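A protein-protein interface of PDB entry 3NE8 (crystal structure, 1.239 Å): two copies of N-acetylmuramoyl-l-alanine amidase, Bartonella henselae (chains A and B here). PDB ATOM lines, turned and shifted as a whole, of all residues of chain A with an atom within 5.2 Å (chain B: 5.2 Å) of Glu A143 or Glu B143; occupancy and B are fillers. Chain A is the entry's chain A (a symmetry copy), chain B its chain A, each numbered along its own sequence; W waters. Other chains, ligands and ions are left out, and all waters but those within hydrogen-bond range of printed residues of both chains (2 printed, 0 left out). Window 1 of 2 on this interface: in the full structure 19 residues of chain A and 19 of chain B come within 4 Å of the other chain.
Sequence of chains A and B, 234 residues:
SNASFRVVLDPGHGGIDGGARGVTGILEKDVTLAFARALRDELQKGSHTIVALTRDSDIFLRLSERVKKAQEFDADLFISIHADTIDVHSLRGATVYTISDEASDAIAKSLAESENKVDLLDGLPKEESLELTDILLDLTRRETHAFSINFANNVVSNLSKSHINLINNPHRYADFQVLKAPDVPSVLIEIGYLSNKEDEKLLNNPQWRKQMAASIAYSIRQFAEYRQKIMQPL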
ATOM      1  N   LEU A 139      22.811   4.605  -3.846  1.00  0.00           N
ATOM      2  CA  LEU A 139      22.909   4.036  -2.504  1.00  0.00           C
ATOM      3  C   LEU A 139      22.178   2.697  -2.409  1.00  0.00           C
ATOM      4  O   LEU A 139      22.710   1.733  -1.861  1.00  0.00           O
ATOM      5  CB  LEU A 139      22.356   5.006  -1.458  1.00  0.00           C
ATOM      6  CG  LEU A 139      23.048   6.367  -1.366  1.00  0.00           C
ATOM      7  CD1 LEU A 139      22.344   7.253  -0.350  1.00  0.00           C
ATOM      8  CD2 LEU A 139      24.515   6.194  -1.008  1.00  0.00           C
ATOM      9  N   THR A 140      20.965   2.642  -2.956  1.00  0.00           N
ATOM     10  CA  THR A 140      20.167   1.417  -2.968  1.00  0.00           C
ATOM     11  C   THR A 140      20.926   0.311  -3.680  1.00  0.00           C
ATOM     12  O   THR A 140      20.956  -0.841  -3.232  1.00  0.00           O
ATOM     13  CB  THR A 140      18.827   1.644  -3.682  1.00  0.00           C
ATOM     14  OG1 THR A 140      18.083   2.653  -2.988  1.00  0.00           O
ATOM     15  CG2 THR A 140      18.005   0.353  -3.733  1.00  0.00           C
ATOM     16  N   ARG A 141      21.547   0.676  -4.794  1.00  0.00           N
ATOM     17  CA  ARG A 141      22.363  -0.248  -5.557  1.00  0.00           C
ATOM     18  C   ARG A 141      23.497  -0.830  -4.719  1.00  0.00           C
ATOM     19  O   ARG A 141      23.810  -2.007  -4.820  1.00  0.00           O
ATOM     20  CB  ARG A 141      22.935   0.448  -6.796  1.00  0.00           C
ATOM     21  CG  ARG A 141      21.891   0.722  -7.863  1.00  0.00           C
ATOM     22  CD  ARG A 141      22.485   1.499  -9.028  1.00  0.00           C
ATOM     23  NE  ARG A 141      23.544   0.753  -9.692  1.00  0.00           N
ATOM     24  CZ  ARG A 141      24.712   1.275 -10.052  1.00  0.00           C
ATOM     25  NH1 ARG A 141      24.972   2.554  -9.811  1.00  0.00           N
ATOM     26  NH2 ARG A 141      25.621   0.518 -10.652  1.00  0.00           N
ATOM     27  N   ARG A 142      24.130   0.012  -3.908  1.00  0.00           N
ATOM     28  CA  ARG A 142      25.269  -0.433  -3.109  1.00  0.00           C
ATOM     29  C   ARG A 142      24.812  -1.433  -2.047  1.00  0.00           C
ATOM     30  O   ARG A 142      25.457  -2.454  -1.807  1.00  0.00           O
ATOM     31  CB  ARG A 142      25.979   0.774  -2.484  1.00  0.00           C
ATOM     32  CG  ARG A 142      27.340   0.470  -1.852  1.00  0.00           C
ATOM     33  CD  ARG A 142      27.996   1.746  -1.334  1.00  0.00           C
ATOM     34  NE  ARG A 142      27.201   2.352  -0.271  1.00  0.00           N
ATOM     35  CZ  ARG A 142      27.272   3.628   0.098  1.00  0.00           C
ATOM     36  NH1 ARG A 142      28.110   4.467  -0.508  1.00  0.00           N
ATOM     37  NH2 ARG A 142      26.496   4.068   1.077  1.00  0.00           N
ATOM     38  N   GLU A 143      23.673  -1.141  -1.439  1.00  0.00           N
ATOM     39  CA  GLU A 143      23.077  -2.035  -0.465  1.00  0.00           C
ATOM     40  C   GLU A 143      22.705  -3.375  -1.105  1.00  0.00           C
ATOM     41  O   GLU A 143      23.000  -4.448  -0.576  1.00  0.00           O
ATOM     42  CB  GLU A 143      21.834  -1.367   0.103  1.00  0.00           C
ATOM     43  CG  GLU A 143      21.294  -2.003   1.348  1.00  0.00           C
ATOM     44  CD  GLU A 143      20.026  -1.333   1.806  1.00  0.00           C
ATOM     45  OE1 GLU A 143      19.277  -0.824   0.943  1.00  0.00           O
ATOM     46  OE2 GLU A 143      19.778  -1.308   3.024  1.00  0.00           O
ATOM     47  N   THR A 144      22.043  -3.310  -2.250  1.00  0.00           N
ATOM     48  CA  THR A 144      21.690  -4.508  -2.994  1.00  0.00           C
ATOM     49  C   THR A 144      22.912  -5.350  -3.304  1.00  0.00           C
ATOM     50  O   THR A 144      22.888  -6.575  -3.174  1.00  0.00           O
ATOM     51  CB  THR A 144      20.961  -4.126  -4.292  1.00  0.00           C
ATOM     52  OG1 THR A 144      19.711  -3.526  -3.934  1.00  0.00           O
ATOM     53  CG2 THR A 144      20.725  -5.333  -5.195  1.00  0.00           C
ATOM     54  N   HIS A 145      23.996  -4.697  -3.705  1.00  0.00           N
ATOM     55  CA  HIS A 145      25.194  -5.430  -4.067  1.00  0.00           C
ATOM     56  C   HIS A 145      25.793  -6.165  -2.865  1.00  0.00           C
ATOM     57  O   HIS A 145      26.260  -7.295  -2.984  1.00  0.00           O
ATOM     58  CB  HIS A 145      26.215  -4.491  -4.698  1.00  0.00           C
ATOM     59  CG  HIS A 145      27.285  -5.211  -5.442  1.00  0.00           C
ATOM     60  ND1 HIS A 145      28.625  -5.010  -5.205  1.00  0.00           N
ATOM     61  CD2 HIS A 145      27.207  -6.152  -6.413  1.00  0.00           C
ATOM     62  CE1 HIS A 145      29.329  -5.791  -6.005  1.00  0.00           C
ATOM     63  NE2 HIS A 145      28.493  -6.495  -6.746  1.00  0.00           N
ATOM     64  N   ALA A 146      25.780  -5.519  -1.709  1.00  0.00           N
ATOM     65  CA  ALA A 146      26.257  -6.172  -0.492  1.00  0.00           C
ATOM     66  C   ALA A 146      25.491  -7.472  -0.254  1.00  0.00           C
ATOM     67  O   ALA A 146      26.075  -8.494   0.094  1.00  0.00           O
ATOM     68  CB  ALA A 146      26.130  -5.246   0.707  1.00  0.00           C
ATOM     69  N   PHE A 147      24.177  -7.444  -0.479  1.00  0.00           N
ATOM     70  CA  PHE A 147      23.358  -8.640  -0.315  1.00  0.00           C
ATOM     71  C   PHE A 147      23.675  -9.693  -1.371  1.00  0.00           C
ATOM     72  O   PHE A 147      23.769 -10.871  -1.051  1.00  0.00           O
ATOM     73  CB  PHE A 147      21.868  -8.293  -0.341  1.00  0.00           C
ATOM     74  CG  PHE A 147      21.379  -7.628   0.910  1.00  0.00           C
ATOM     75  CD1 PHE A 147      21.679  -8.163   2.154  1.00  0.00           C
ATOM     76  CD2 PHE A 147      20.607  -6.481   0.853  1.00  0.00           C
ATOM     77  CE1 PHE A 147      21.221  -7.552   3.316  1.00  0.00           C
ATOM     78  CE2 PHE A 147      20.136  -5.871   2.006  1.00  0.00           C
ATOM     79  CZ  PHE A 147      20.453  -6.406   3.242  1.00  0.00           C
ATOM     80  N   LEU B 139      18.516   5.424   5.020  1.00  0.00           N
ATOM     81  CA  LEU B 139      19.031   4.393   4.123  1.00  0.00           C
ATOM     82  C   LEU B 139      20.441   3.957   4.521  1.00  0.00           C
ATOM     83  O   LEU B 139      20.735   2.764   4.572  1.00  0.00           O
ATOM     84  CB  LEU B 139      19.026   4.879   2.672  1.00  0.00           C
ATOM     85  CG  LEU B 139      17.665   5.268   2.095  1.00  0.00           C
ATOM     86  CD1 LEU B 139      17.822   5.808   0.682  1.00  0.00           C
ATOM     87  CD2 LEU B 139      16.719   4.077   2.115  1.00  0.00           C
ATOM     88  N   THR B 140      21.302   4.930   4.813  1.00  0.00           N
ATOM     89  CA  THR B 140      22.673   4.658   5.241  1.00  0.00           C
ATOM     90  C   THR B 140      22.664   3.804   6.498  1.00  0.00           C
ATOM     91  O   THR B 140      23.440   2.852   6.634  1.00  0.00           O
ATOM     92  CB  THR B 140      23.427   5.964   5.529  1.00  0.00           C
ATOM     93  OG1 THR B 140      23.481   6.754   4.335  1.00  0.00           O
ATOM     94  CG2 THR B 140      24.851   5.683   6.017  1.00  0.00           C
ATOM     95  N   ARG B 141      21.770   4.154   7.413  1.00  0.00           N
ATOM     96  CA  ARG B 141      21.595   3.403   8.641  1.00  0.00           C
ATOM     97  C   ARG B 141      21.243   1.944   8.371  1.00  0.00           C
ATOM     98  O   ARG B 141      21.724   1.048   9.047  1.00  0.00           O
ATOM     99  CB  ARG B 141      20.510   4.049   9.507  1.00  0.00           C
ATOM    100  CG  ARG B 141      20.946   5.361  10.134  1.00  0.00           C
ATOM    101  CD  ARG B 141      19.806   6.012  10.902  1.00  0.00           C
ATOM    102  NE  ARG B 141      19.352   5.176  12.005  1.00  0.00           N
ATOM    103  CZ  ARG B 141      18.075   4.940  12.286  1.00  0.00           C
ATOM    104  NH1 ARG B 141      17.119   5.480  11.540  1.00  0.00           N
ATOM    105  NH2 ARG B 141      17.753   4.164  13.312  1.00  0.00           N
ATOM    106  N   ARG B 142      20.376   1.714   7.390  1.00  0.00           N
ATOM    107  CA  ARG B 142      19.927   0.356   7.091  1.00  0.00           C
ATOM    108  C   ARG B 142      21.084  -0.474   6.538  1.00  0.00           C
ATOM    109  O   ARG B 142      21.274  -1.635   6.904  1.00  0.00           O
ATOM    110  CB  ARG B 142      18.740   0.394   6.120  1.00  0.00           C
ATOM    111  CG  ARG B 142      18.005  -0.938   5.942  1.00  0.00           C
ATOM    112  CD  ARG B 142      16.798  -0.774   5.025  1.00  0.00           C
ATOM    113  NE  ARG B 142      17.208  -0.375   3.683  1.00  0.00           N
ATOM    114  CZ  ARG B 142      16.420   0.222   2.793  1.00  0.00           C
ATOM    115  NH1 ARG B 142      15.153   0.505   3.087  1.00  0.00           N
ATOM    116  NH2 ARG B 142      16.905   0.542   1.602  1.00  0.00           N
ATOM    117  N   GLU B 143      21.874   0.147   5.676  1.00  0.00           N
ATOM    118  CA  GLU B 143      23.056  -0.489   5.127  1.00  0.00           C
ATOM    119  C   GLU B 143      24.066  -0.816   6.230  1.00  0.00           C
ATOM    120  O   GLU B 143      24.605  -1.921   6.306  1.00  0.00           O
ATOM    121  CB  GLU B 143      23.682   0.454   4.111  1.00  0.00           C
ATOM    122  CG  GLU B 143      24.707  -0.177   3.219  1.00  0.00           C
ATOM    123  CD  GLU B 143      25.331   0.834   2.294  1.00  0.00           C
ATOM    124  OE1 GLU B 143      25.433   2.017   2.686  1.00  0.00           O
ATOM    125  OE2 GLU B 143      25.716   0.452   1.175  1.00  0.00           O
ATOM    126  N   THR B 144      24.330   0.160   7.087  1.00  0.00           N
ATOM    127  CA  THR B 144      25.218  -0.042   8.219  1.00  0.00           C
ATOM    128  C   THR B 144      24.762  -1.199   9.085  1.00  0.00           C
ATOM    129  O   THR B 144      25.569  -2.021   9.523  1.00  0.00           O
ATOM    130  CB  THR B 144      25.308   1.246   9.053  1.00  0.00           C
ATOM    131  OG1 THR B 144      25.945   2.246   8.250  1.00  0.00           O
ATOM    132  CG2 THR B 144      26.086   1.038  10.349  1.00  0.00           C
ATOM    133  N   HIS B 145      23.459  -1.281   9.327  1.00  0.00           N
ATOM    134  CA  HIS B 145      22.944  -2.331  10.184  1.00  0.00           C
ATOM    135  C   HIS B 145      23.157  -3.718   9.572  1.00  0.00           C
ATOM    136  O   HIS B 145      23.488  -4.673  10.270  1.00  0.00           O
ATOM    137  CB  HIS B 145      21.470  -2.088  10.487  1.00  0.00           C
ATOM    138  CG  HIS B 145      20.977  -2.877  11.650  1.00  0.00           C
ATOM    139  ND1 HIS B 145      19.874  -3.695  11.585  1.00  0.00           N
ATOM    140  CD2 HIS B 145      21.457  -2.983  12.912  1.00  0.00           C
ATOM    141  CE1 HIS B 145      19.688  -4.268  12.760  1.00  0.00           C
ATOM    142  NE2 HIS B 145      20.635  -3.855  13.582  1.00  0.00           N
ATOM    143  N   ALA B 146      22.964  -3.826   8.266  1.00  0.00           N
ATOM    144  CA  ALA B 146      23.222  -5.091   7.582  1.00  0.00           C
ATOM    145  C   ALA B 146      24.659  -5.544   7.832  1.00  0.00           C
ATOM    146  O   ALA B 146      24.914  -6.716   8.093  1.00  0.00           O
ATOM    147  CB  ALA B 146      22.946  -4.969   6.092  1.00  0.00           C
ATOM    148  N   PHE B 147      25.601  -4.602   7.787  1.00  0.00           N
ATOM    149  CA  PHE B 147      27.001  -4.922   8.044  1.00  0.00           C
ATOM    150  C   PHE B 147      27.235  -5.310   9.500  1.00  0.00           C
ATOM    151  O   PHE B 147      27.956  -6.260   9.772  1.00  0.00           O
ATOM    152  CB  PHE B 147      27.912  -3.758   7.650  1.00  0.00           C
ATOM    153  CG  PHE B 147      28.085  -3.599   6.170  1.00  0.00           C
ATOM    154  CD1 PHE B 147      28.408  -4.691   5.378  1.00  0.00           C
ATOM    155  CD2 PHE B 147      27.945  -2.363   5.565  1.00  0.00           C
ATOM    156  CE1 PHE B 147      28.576  -4.544   4.006  1.00  0.00           C
ATOM    157  CE2 PHE B 147      28.122  -2.204   4.199  1.00  0.00           C
ATOM    158  CZ  PHE B 147      28.431  -3.303   3.417  1.00  0.00           C
HETATM  159  O   HOH W   1      20.362  -3.261   4.612  1.00  0.00           O
HETATM  160  O   HOH W   2      26.770  -1.873   0.775  1.00  0.00           O
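Arg A142 touches Glu B143, and with the chains exchanged Glu A143 touches Arg B142.
Glu B143 touches its own counterpart, Glu A143.
Of the 3 pairs that touch across the chains among the printed residues, 3 have their exchanged pair printed and touching as well.
Water W1 lies within hydrogen-bond range of the side-chain carboxylate of Glu A143 and the backbone carbonyl oxygen of Arg B142.
Water W2 bridges OE2 of Glu B143 and O of Arg A142.
Of the printed residues of chain B, Glu A143 touches Arg B142 and Glu B143.
Printed residues of chain A within 4 Å of Glu B143: Arg A142 and Glu A143.
Of the printed residues of chain A, Arg B142 touches Glu A143 (2.8 Å).
Printed residues of chain B within 4 Å of Arg A142: Glu B143 (2.8 Å).
OE2 of Glu A143 touches N of Glu B143, at 3.7 Å.
Of the 9 printed residues of chain A, 2 touch a printed residue of chain B.
The side-chain carboxylate of Glu A143 lies within salt-bridge range of the guanidinium group of Arg B142.
The side-chain carboxylate (OE2) of Glu B143 lies within salt-bridge range of the guanidinium group (NE) of Arg A142 (2.8 Å).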
